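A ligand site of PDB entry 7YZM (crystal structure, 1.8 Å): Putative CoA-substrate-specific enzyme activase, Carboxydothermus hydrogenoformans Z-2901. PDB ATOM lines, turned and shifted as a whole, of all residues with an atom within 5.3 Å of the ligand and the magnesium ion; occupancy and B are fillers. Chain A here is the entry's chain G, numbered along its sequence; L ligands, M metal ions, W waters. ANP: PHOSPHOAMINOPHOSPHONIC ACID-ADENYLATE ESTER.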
ATOM      1  N   ASP A   6     -15.725  10.735 -16.098  1.00  0.00           N
ATOM      2  CA  ASP A   6     -14.690   9.707 -15.929  1.00  0.00           C
ATOM      3  C   ASP A   6     -15.360   8.429 -15.433  1.00  0.00           C
ATOM      4  O   ASP A   6     -15.705   8.303 -14.253  1.00  0.00           O
ATOM      5  CB  ASP A   6     -13.629  10.201 -14.947  1.00  0.00           C
ATOM      6  CG  ASP A   6     -12.582   9.161 -14.626  1.00  0.00           C
ATOM      7  OD1 ASP A   6     -12.562   8.067 -15.238  1.00  0.00           O
ATOM      8  OD2 ASP A   6     -11.763   9.450 -13.718  1.00  0.00           O
ATOM      9  N   GLY A   8     -14.767   5.155 -14.489  1.00  0.00           N
ATOM     10  CA  GLY A   8     -13.709   4.274 -14.074  1.00  0.00           C
ATOM     11  C   GLY A   8     -14.191   2.869 -13.758  1.00  0.00           C
ATOM     12  O   GLY A   8     -15.386   2.590 -13.682  1.00  0.00           O
ATOM     13  N   SER A   9     -13.216   1.975 -13.566  1.00  0.00           N
ATOM     14  CA  SER A   9     -13.538   0.579 -13.297  1.00  0.00           C
ATOM     15  C   SER A   9     -14.332   0.406 -12.023  1.00  0.00           C
ATOM     16  O   SER A   9     -15.155  -0.519 -11.917  1.00  0.00           O
ATOM     17  CB  SER A   9     -12.238  -0.238 -13.231  1.00  0.00           C
ATOM     18  OG  SER A   9     -11.522   0.063 -12.043  1.00  0.00           O
ATOM     19  N   THR A  10     -14.114   1.272 -11.030  1.00  0.00           N
ATOM     20  CA  THR A  10     -14.782   1.189  -9.735  1.00  0.00           C
ATOM     21  C   THR A  10     -15.745   2.331  -9.477  1.00  0.00           C
ATOM     22  O   THR A  10     -16.863   2.101  -9.010  1.00  0.00           O
ATOM     23  CB  THR A  10     -13.742   1.155  -8.604  1.00  0.00           C
ATOM     24  OG1 THR A  10     -12.835   0.070  -8.810  1.00  0.00           O
ATOM     25  CG2 THR A  10     -14.431   0.973  -7.267  1.00  0.00           C
ATOM     26  N   ASN A  11     -15.324   3.570  -9.756  1.00  0.00           N
ATOM     27  CA  ASN A  11     -16.138   4.745  -9.512  1.00  0.00           C
ATOM     28  C   ASN A  11     -16.252   5.569 -10.780  1.00  0.00           C
ATOM     29  O   ASN A  11     -15.351   5.599 -11.612  1.00  0.00           O
ATOM     30  CB  ASN A  11     -15.559   5.613  -8.404  1.00  0.00           C
ATOM     31  CG  ASN A  11     -15.469   4.882  -7.111  1.00  0.00           C
ATOM     32  OD1 ASN A  11     -16.480   4.526  -6.519  1.00  0.00           O
ATOM     33  ND2 ASN A  11     -14.249   4.570  -6.690  1.00  0.00           N
ATOM     34  N   LYS A  13     -17.125   9.584 -12.103  1.00  0.00           N
ATOM     35  CA  LYS A  13     -16.974  10.956 -11.640  1.00  0.00           C
ATOM     36  C   LYS A  13     -17.405  11.915 -12.738  1.00  0.00           C
ATOM     37  O   LYS A  13     -17.155  11.676 -13.923  1.00  0.00           O
ATOM     38  CB  LYS A  13     -15.512  11.269 -11.258  1.00  0.00           C
ATOM     39  CG  LYS A  13     -14.884  10.293 -10.270  1.00  0.00           C
ATOM     40  CD  LYS A  13     -14.277   9.100 -11.010  1.00  0.00           C
ATOM     41  CE  LYS A  13     -13.400   8.255 -10.120  1.00  0.00           C
ATOM     42  NZ  LYS A  13     -12.847   7.107 -10.892  1.00  0.00           N
ATOM     43  N   THR A  30     -19.461   2.793 -10.029  1.00  0.00           N
ATOM     44  CA  THR A  30     -19.801   2.399 -11.391  1.00  0.00           C
ATOM     45  C   THR A  30     -20.672   1.160 -11.425  1.00  0.00           C
ATOM     46  O   THR A  30     -21.508   1.008 -12.327  1.00  0.00           O
ATOM     47  CB  THR A  30     -18.532   2.133 -12.206  1.00  0.00           C
ATOM     48  OG1 THR A  30     -17.644   3.246 -12.094  1.00  0.00           O
ATOM     49  CG2 THR A  30     -18.912   1.964 -13.645  1.00  0.00           C
ATOM     50  N   TYR A  56     -12.608   3.622 -18.514  1.00  0.00           N
ATOM     51  CA  TYR A  56     -13.021   2.387 -19.194  1.00  0.00           C
ATOM     52  C   TYR A  56     -14.342   2.547 -19.928  1.00  0.00           C
ATOM     53  O   TYR A  56     -14.496   2.082 -21.060  1.00  0.00           O
ATOM     54  CB  TYR A  56     -13.140   1.230 -18.186  1.00  0.00           C
ATOM     55  CG  TYR A  56     -11.857   0.486 -17.986  1.00  0.00           C
ATOM     56  CD1 TYR A  56     -11.375  -0.381 -18.952  1.00  0.00           C
ATOM     57  CD2 TYR A  56     -11.101   0.683 -16.834  1.00  0.00           C
ATOM     58  CE1 TYR A  56     -10.169  -1.048 -18.769  1.00  0.00           C
ATOM     59  CE2 TYR A  56      -9.890   0.032 -16.652  1.00  0.00           C
ATOM     60  CZ  TYR A  56      -9.441  -0.832 -17.622  1.00  0.00           C
ATOM     61  OH  TYR A  56      -8.237  -1.493 -17.447  1.00  0.00           O
ATOM     62  N   GLU A  69      -7.847   8.549 -20.219  1.00  0.00           N
ATOM     63  CA  GLU A  69      -7.621   9.061 -18.875  1.00  0.00           C
ATOM     64  C   GLU A  69      -6.179   9.508 -18.666  1.00  0.00           C
ATOM     65  O   GLU A  69      -5.918  10.261 -17.728  1.00  0.00           O
ATOM     66  CB  GLU A  69      -7.993   7.986 -17.849  1.00  0.00           C
ATOM     67  CG  GLU A  69      -7.269   6.650 -18.009  1.00  0.00           C
ATOM     68  CD  GLU A  69      -7.989   5.476 -17.351  1.00  0.00           C
ATOM     69  OE1 GLU A  69      -7.752   5.227 -16.139  1.00  0.00           O
ATOM     70  OE2 GLU A  69      -8.788   4.796 -18.025  1.00  0.00           O
ATOM     71  N   ASP A  89      -1.261   7.976 -10.751  1.00  0.00           N
ATOM     72  CA  ASP A  89      -2.699   7.742 -10.623  1.00  0.00           C
ATOM     73  C   ASP A  89      -2.855   6.272 -10.261  1.00  0.00           C
ATOM     74  O   ASP A  89      -2.462   5.405 -11.058  1.00  0.00           O
ATOM     75  CB  ASP A  89      -3.399   8.122 -11.932  1.00  0.00           C
ATOM     76  CG  ASP A  89      -4.857   7.638 -12.040  1.00  0.00           C
ATOM     77  OD1 ASP A  89      -5.338   6.806 -11.229  1.00  0.00           O
ATOM     78  OD2 ASP A  89      -5.526   8.086 -12.987  1.00  0.00           O
ATOM     79  N   LEU A  90      -3.348   5.987  -9.061  1.00  0.00           N
ATOM     80  CA  LEU A  90      -3.661   4.620  -8.657  1.00  0.00           C
ATOM     81  C   LEU A  90      -5.183   4.492  -8.599  1.00  0.00           C
ATOM     82  O   LEU A  90      -5.839   5.096  -7.751  1.00  0.00           O
ATOM     83  CB  LEU A  90      -3.014   4.264  -7.320  1.00  0.00           C
ATOM     84  CG  LEU A  90      -3.322   2.839  -6.860  1.00  0.00           C
ATOM     85  CD1 LEU A  90      -2.888   1.799  -7.922  1.00  0.00           C
ATOM     86  CD2 LEU A  90      -2.716   2.502  -5.501  1.00  0.00           C
ATOM     87  N   GLY A  91      -5.736   3.717  -9.528  1.00  0.00           N
ATOM     88  CA  GLY A  91      -7.147   3.412  -9.547  1.00  0.00           C
ATOM     89  C   GLY A  91      -7.403   1.991  -9.080  1.00  0.00           C
ATOM     90  O   GLY A  91      -6.554   1.328  -8.490  1.00  0.00           O
ATOM     91  N   GLY A  92      -8.626   1.511  -9.352  1.00  0.00           N
ATOM     92  CA  GLY A  92      -8.994   0.175  -8.915  1.00  0.00           C
ATOM     93  C   GLY A  92      -8.409  -0.922  -9.781  1.00  0.00           C
ATOM     94  O   GLY A  92      -8.163  -2.026  -9.278  1.00  0.00           O
ATOM     95  N   GLN A  93      -8.201  -0.653 -11.056  1.00  0.00           N
ATOM     96  CA  GLN A  93      -7.675  -1.658 -11.982  1.00  0.00           C
ATOM     97  C   GLN A  93      -6.308  -1.321 -12.551  1.00  0.00           C
ATOM     98  O   GLN A  93      -5.480  -2.218 -12.728  1.00  0.00           O
ATOM     99  CB  GLN A  93      -8.685  -1.892 -13.118  1.00  0.00           C
ATOM    100  CG  GLN A  93      -8.150  -2.560 -14.398  1.00  0.00           C
ATOM    101  CD  GLN A  93      -7.758  -4.024 -14.242  1.00  0.00           C
ATOM    102  OE1 GLN A  93      -7.103  -4.588 -15.124  1.00  0.00           O
ATOM    103  NE2 GLN A  93      -8.165  -4.656 -13.142  1.00  0.00           N
ATOM    104  N   ASP A  94      -6.032  -0.054 -12.871  1.00  0.00           N
ATOM    105  CA  ASP A  94      -4.777   0.337 -13.481  1.00  0.00           C
ATOM    106  C   ASP A  94      -4.021   1.332 -12.600  1.00  0.00           C
ATOM    107  O   ASP A  94      -4.620   2.140 -11.886  1.00  0.00           O
ATOM    108  CB  ASP A  94      -4.983   0.995 -14.858  1.00  0.00           C
ATOM    109  CG  ASP A  94      -5.638   0.077 -15.864  1.00  0.00           C
ATOM    110  OD1 ASP A  94      -6.888   0.043 -15.897  1.00  0.00           O
ATOM    111  OD2 ASP A  94      -4.917  -0.613 -16.625  1.00  0.00           O
ATOM    112  N   LYS A  96      -0.960   4.296 -13.258  1.00  0.00           N
ATOM    113  CA  LYS A  96      -0.479   5.136 -14.342  1.00  0.00           C
ATOM    114  C   LYS A  96       0.566   6.084 -13.786  1.00  0.00           C
ATOM    115  O   LYS A  96       0.340   6.717 -12.752  1.00  0.00           O
ATOM    116  CB  LYS A  96      -1.623   5.925 -14.987  1.00  0.00           C
ATOM    117  CG  LYS A  96      -2.919   5.140 -15.274  1.00  0.00           C
ATOM    118  CD  LYS A  96      -3.754   4.906 -14.014  1.00  0.00           C
ATOM    119  CE  LYS A  96      -5.259   4.872 -14.292  1.00  0.00           C
ATOM    120  NZ  LYS A  96      -6.060   4.436 -13.101  1.00  0.00           N
ATOM    121  N   GLY A 120      -5.576  -1.732  -6.833  1.00  0.00           N
ATOM    122  CA  GLY A 120      -6.494  -0.905  -6.073  1.00  0.00           C
ATOM    123  C   GLY A 120      -7.669  -1.691  -5.523  1.00  0.00           C
ATOM    124  O   GLY A 120      -7.978  -1.622  -4.329  1.00  0.00           O
ATOM    125  N   ARG A 121      -8.343  -2.438  -6.397  1.00  0.00           N
ATOM    126  CA  ARG A 121      -9.488  -3.248  -5.983  1.00  0.00           C
ATOM    127  C   ARG A 121      -9.085  -4.268  -4.925  1.00  0.00           C
ATOM    128  O   ARG A 121      -9.849  -4.537  -3.982  1.00  0.00           O
ATOM    129  CB  ARG A 121     -10.085  -3.944  -7.211  1.00  0.00           C
ATOM    130  CG  ARG A 121     -11.160  -4.957  -6.912  1.00  0.00           C
ATOM    131  CD  ARG A 121     -12.488  -4.316  -6.548  1.00  0.00           C
ATOM    132  NE  ARG A 121     -13.506  -5.346  -6.348  1.00  0.00           N
ATOM    133  CZ  ARG A 121     -14.421  -5.340  -5.386  1.00  0.00           C
ATOM    134  NH1 ARG A 121     -14.459  -4.350  -4.508  1.00  0.00           N
ATOM    135  NH2 ARG A 121     -15.292  -6.336  -5.300  1.00  0.00           N
ATOM    136  N   LEU A 123      -6.698  -3.998  -2.653  1.00  0.00           N
ATOM    137  CA  LEU A 123      -6.593  -3.310  -1.369  1.00  0.00           C
ATOM    138  C   LEU A 123      -7.977  -3.049  -0.789  1.00  0.00           C
ATOM    139  O   LEU A 123      -8.208  -3.261   0.406  1.00  0.00           O
ATOM    140  CB  LEU A 123      -5.822  -2.004  -1.533  1.00  0.00           C
ATOM    141  CG  LEU A 123      -4.340  -2.143  -1.899  1.00  0.00           C
ATOM    142  CD1 LEU A 123      -3.765  -0.799  -2.290  1.00  0.00           C
ATOM    143  CD2 LEU A 123      -3.539  -2.769  -0.767  1.00  0.00           C
ATOM    144  N   GLU A 124      -8.920  -2.634  -1.638  1.00  0.00           N
ATOM    145  CA  GLU A 124     -10.272  -2.347  -1.171  1.00  0.00           C
ATOM    146  C   GLU A 124     -10.907  -3.599  -0.574  1.00  0.00           C
ATOM    147  O   GLU A 124     -11.503  -3.560   0.509  1.00  0.00           O
ATOM    148  CB  GLU A 124     -11.117  -1.800  -2.329  1.00  0.00           C
ATOM    149  CG  GLU A 124     -12.567  -1.453  -1.952  1.00  0.00           C
ATOM    150  CD  GLU A 124     -13.412  -0.992  -3.137  1.00  0.00           C
ATOM    151  OE1 GLU A 124     -13.131  -1.389  -4.295  1.00  0.00           O
ATOM    152  OE2 GLU A 124     -14.385  -0.241  -2.906  1.00  0.00           O
ATOM    153  N   GLY A 202      -5.883   9.800  -7.918  1.00  0.00           N
ATOM    154  CA  GLY A 202      -6.781   8.670  -7.965  1.00  0.00           C
ATOM    155  C   GLY A 202      -7.220   8.242  -6.566  1.00  0.00           C
ATOM    156  O   GLY A 202      -6.684   8.677  -5.550  1.00  0.00           O
ATOM    157  N   GLY A 203      -8.210   7.355  -6.542  1.00  0.00           N
ATOM    158  CA  GLY A 203      -8.723   6.869  -5.275  1.00  0.00           C
ATOM    159  C   GLY A 203      -7.675   6.232  -4.384  1.00  0.00           C
ATOM    160  O   GLY A 203      -7.769   6.319  -3.152  1.00  0.00           O
ATOM    161  N   GLY A 204      -6.681   5.574  -4.980  1.00  0.00           N
ATOM    162  CA  GLY A 204      -5.624   4.965  -4.184  1.00  0.00           C
ATOM    163  C   GLY A 204      -4.877   5.960  -3.325  1.00  0.00           C
ATOM    164  O   GLY A 204      -4.343   5.601  -2.274  1.00  0.00           O
ATOM    165  N   LYS A 206      -6.081   8.144  -1.531  1.00  0.00           N
ATOM    166  CA  LYS A 206      -6.862   8.505  -0.351  1.00  0.00           C
ATOM    167  C   LYS A 206      -6.526   7.640   0.847  1.00  0.00           C
ATOM    168  O   LYS A 206      -7.060   7.897   1.931  1.00  0.00           O
ATOM    169  CB  LYS A 206      -8.354   8.416  -0.673  1.00  0.00           C
ATOM    170  CG  LYS A 206      -8.793   9.391  -1.745  1.00  0.00           C
ATOM    171  CD  LYS A 206     -10.240   9.192  -2.158  1.00  0.00           C
ATOM    172  CE  LYS A 206     -11.172  10.041  -1.317  1.00  0.00           C
ATOM    173  NZ  LYS A 206     -12.073  10.879  -2.145  1.00  0.00           N
ATOM    174  N   TYR A 207      -5.662   6.637   0.686  1.00  0.00           N
ATOM    175  CA  TYR A 207      -5.116   5.862   1.801  1.00  0.00           C
ATOM    176  C   TYR A 207      -3.945   6.615   2.427  1.00  0.00           C
ATOM    177  O   TYR A 207      -2.827   6.556   1.895  1.00  0.00           O
ATOM    178  CB  TYR A 207      -4.639   4.490   1.328  1.00  0.00           C
ATOM    179  CG  TYR A 207      -5.712   3.543   0.855  1.00  0.00           C
ATOM    180  CD1 TYR A 207      -6.807   3.255   1.652  1.00  0.00           C
ATOM    181  CD2 TYR A 207      -5.619   2.913  -0.382  1.00  0.00           C
ATOM    182  CE1 TYR A 207      -7.782   2.378   1.227  1.00  0.00           C
ATOM    183  CE2 TYR A 207      -6.596   2.042  -0.815  1.00  0.00           C
ATOM    184  CZ  TYR A 207      -7.668   1.778  -0.003  1.00  0.00           C
ATOM    185  OH  TYR A 207      -8.645   0.903  -0.414  1.00  0.00           O
ATOM    186  N   SER A 229     -10.107  11.851  -6.311  1.00  0.00           N
ATOM    187  CA  SER A 229     -11.009  11.048  -7.136  1.00  0.00           C
ATOM    188  C   SER A 229     -11.350  11.713  -8.459  1.00  0.00           C
ATOM    189  O   SER A 229     -11.618  11.020  -9.439  1.00  0.00           O
ATOM    190  CB  SER A 229     -12.296  10.742  -6.381  1.00  0.00           C
ATOM    191  OG  SER A 229     -12.091   9.779  -5.360  1.00  0.00           O
HETATM  192  PG  ANP L   1      -9.430   2.752 -12.928  1.00  0.00           P
HETATM  193  O1G ANP L   1     -10.196   2.356 -14.141  1.00  0.00           O
HETATM  194  O2G ANP L   1      -8.293   1.708 -12.638  1.00  0.00           O
HETATM  195  O3G ANP L   1      -8.795   4.185 -13.149  1.00  0.00           O
HETATM  196  PB  ANP L   1     -11.195   4.019 -10.904  1.00  0.00           P
HETATM  197  O1B ANP L   1     -12.658   3.728 -10.752  1.00  0.00           O
HETATM  198  O2B ANP L   1     -10.935   5.329 -11.696  1.00  0.00           O
HETATM  199  N3B ANP L   1     -10.544   2.675 -11.652  1.00  0.00           N
HETATM  200  PA  ANP L   1     -10.573   5.280  -8.434  1.00  0.00           P
HETATM  201  O1A ANP L   1     -11.965   5.703  -8.186  1.00  0.00           O
HETATM  202  O2A ANP L   1      -9.625   6.388  -8.879  1.00  0.00           O
HETATM  203  O3A ANP L   1     -10.526   4.066  -9.482  1.00  0.00           O
HETATM  204  O5' ANP L   1      -9.988   4.675  -7.109  1.00  0.00           O
HETATM  205  C5' ANP L   1     -10.505   3.463  -6.565  1.00  0.00           C
HETATM  206  C4' ANP L   1      -9.657   2.974  -5.427  1.00  0.00           C
HETATM  207  O4' ANP L   1      -9.718   3.876  -4.307  1.00  0.00           O
HETATM  208  C3' ANP L   1     -10.107   1.648  -4.829  1.00  0.00           C
HETATM  209  O3' ANP L   1      -9.672   0.535  -5.604  1.00  0.00           O
HETATM  210  C2' ANP L   1      -9.483   1.677  -3.425  1.00  0.00           C
HETATM  211  O2' ANP L   1      -8.243   0.973  -3.378  1.00  0.00           O
HETATM  212  C1' ANP L   1      -9.218   3.170  -3.182  1.00  0.00           C
HETATM  213  N9  ANP L   1      -9.834   3.689  -1.962  1.00  0.00           N
HETATM  214  C8  ANP L   1      -9.236   4.481  -1.016  1.00  0.00           C
HETATM  215  N7  ANP L   1     -10.006   4.792  -0.002  1.00  0.00           N
HETATM  216  C5  ANP L   1     -11.201   4.146  -0.290  1.00  0.00           C
HETATM  217  C6  ANP L   1     -12.421   4.063   0.394  1.00  0.00           C
HETATM  218  N6  ANP L   1     -12.672   4.674   1.556  1.00  0.00           N
HETATM  219  N1  ANP L   1     -13.415   3.333  -0.170  1.00  0.00           N
HETATM  220  C2  ANP L   1     -13.174   2.719  -1.333  1.00  0.00           C
HETATM  221  N3  ANP L   1     -12.059   2.721  -2.071  1.00  0.00           N
HETATM  222  C4  ANP L   1     -11.103   3.462  -1.492  1.00  0.00           C
HETATM  223 MG    MG M   1      -9.497   6.066 -12.861  1.00  0.00          MG
HETATM  224  O   HOH W   1      -9.937   8.918  -9.953  1.00  0.00           O
HETATM  225  O   HOH W   2      -7.624   2.502 -16.077  1.00  0.00           O
HETATM  226  O   HOH W   3     -13.659   2.583  -4.384  1.00  0.00           O
HETATM  227  O   HOH W   4     -10.735   3.897 -16.096  1.00  0.00           O
HETATM  228  O   HOH W   5      -8.184   6.345 -11.112  1.00  0.00           O
HETATM  229  O   HOH W   6      -9.540   5.862   2.454  1.00  0.00           O
HETATM  230  O   HOH W   7     -10.351   8.027 -12.384  1.00  0.00           O
HETATM  231  O   HOH W   8     -12.828   7.577  -6.256  1.00  0.00           O
HETATM  232  O   HOH W   9     -15.455   2.221   1.375  1.00  0.00           O
HETATM  233  O   HOH W  10     -11.898  -0.977  -6.326  1.00  0.00           O
HETATM  234  O   HOH W  11     -10.741   6.195 -14.491  1.00  0.00           O
HETATM  235  O   HOH W  12      -7.844   6.773 -13.947  1.00  0.00           O
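Water W7 bridges the side-chain carboxylate (OD2) of Asp 6 (2.4 Å) and the side-chain amino group (NZ) of Lys 13 (3.0 Å). Water W12 lies within hydrogen-bond range of the side-chain carboxylate (OE1) of Glu 69, the side-chain carboxylate (OD2) of Asp 89 and the side-chain amino group (NZ) of Lys 96. Water W6 lies within hydrogen-bond range of N7 of the ligand and O of Lys 206. Water W10 lies within hydrogen-bond range of the side-chain carboxylate of Glu 124 (2.4 Å), an oxygen (O3') of the ligand (2.8 Å) and the side-chain hydroxyl of Thr 10 (2.9 Å). Water W8 lies within hydrogen-bond range of the side-chain hydroxyl (OG) of Ser 229, an oxygen (O1A) of the ligand and the side-chain amide nitrogen (ND2) of Asn 11. Water W2 lies within hydrogen-bond range of OD1 of Asp 94 (2.6 Å), OE1 of Glu 69 (2.7 Å) and O1G of the ligand (3.2 Å).
An oxygen (O3G) of the ligand sits close to the side-chain carboxylate (OE1) of Glu 69, at 3.3 Å. Gly 8 touches the ligand (C to O1B, 3.5 Å). Tyr 56 touches the ligand. Gly 91 touches the ligand (CA to O3A, 3.4 Å). OE2 of Glu 124 touches C2 of the ligand, 3.6 Å away. Gly 202 touches the ligand. N of Gly 204 touches O4' of the ligand (3.5 Å). Hydrophobic or aromatic side chains within 4 Å of the ligand: Tyr 56 and Tyr 207. The nearest printed residue that does not touch the ligand is Lys 206 (4.04 Å).
An oxygen (O1A) of the ligand lies within salt-bridge range of the side-chain amino group of Lys 13 (3.2 Å). The side-chain amino group (NZ) of Lys 96 is in salt-bridge range of an oxygen (O2G) of the ligand (3.6 Å). The backbone carbonyl oxygen (O) of Gly 120 is in hydrogen-bond range of an oxygen (O2') of the ligand (2.8 Å). An oxygen (O1G) of the ligand sits at hydrogen-bond distance from the backbone NH of Ser 9 (3.1 Å). OG of Ser 9 is in hydrogen-bond range of N3B of the ligand, 2.8 Å away. O2G of the ligand is in hydrogen-bond range of N of Gln 93, 2.8 Å away. O1B of the ligand is in hydrogen-bond range of N of Asn 11, at 2.9 Å. An oxygen (O1A) of the ligand is in hydrogen-bond range of the side-chain amide nitrogen (ND2) of Asn 11 (3.0 Å). An oxygen (O1B) of the ligand sits at hydrogen-bond distance from the backbone NH of Thr 10 (2.9 Å). An oxygen (O2G) of the ligand is in hydrogen-bond range of the backbone NH (N) of Asp 94 (2.9 Å). The backbone NH (N) of Gly 203 sits at hydrogen-bond distance from an oxygen (O2A) of the ligand (2.9 Å). The side-chain hydroxyl (OH) of Tyr 207 is in hydrogen-bond range of an oxygen (O2') of the ligand, at 3.0 Å. O3A of the ligand lies within hydrogen-bond range of N of Gly 92. The backbone NH of Arg 121 is in hydrogen-bond range of an oxygen (O3') of the ligand (3.4 Å).
The magnesium ion is bound by O2B of the ligand (2.0 Å), O3G of the ligand (2.0 Å), water W11 (2.1 Å), water W12 (2.1 Å), water W7 (2.2 Å) and water W5 (2.2 Å).
NZ of Lys 13 lies within hydrogen-bond range of O of Asn 11. The side-chain amino group (NZ) of Lys 96 lies within hydrogen-bond range of the backbone carbonyl oxygen (O) of Asp 94 (3.0 Å). The side-chain amino group (NZ) of Lys 96 lies within salt-bridge range of the side-chain carboxylate (OE1) of Glu 69. The side-chain hydroxyl (OG) of Ser 9 is in hydrogen-bond range of the side-chain hydroxyl (OG1) of Thr 10, at 3.5 Å. The backbone carbonyl oxygen (O) of Thr 10 lies within hydrogen-bond range of the backbone NH (N) of Thr 30 (2.9 Å). N of Gly 203 sits at hydrogen-bond distance from O of Leu 90, at 3.5 Å. O of Gly 92 is in hydrogen-bond range of N of Arg 121, 2.9 Å away. The side-chain carboxylate (OE1) of Glu 124 lies within salt-bridge range of the guanidinium group (NH1) of Arg 121 (3.3 Å).
Residues that only touch the magnesium ion: Glu 69 (3.8 Å) and Lys 96 (3.8 Å). Of the 26 residues printed, 2 come within 4 Å of the magnesium ion. The nearest printed residue that does not touch the magnesium ion is Lys 13 (4.02 Å).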
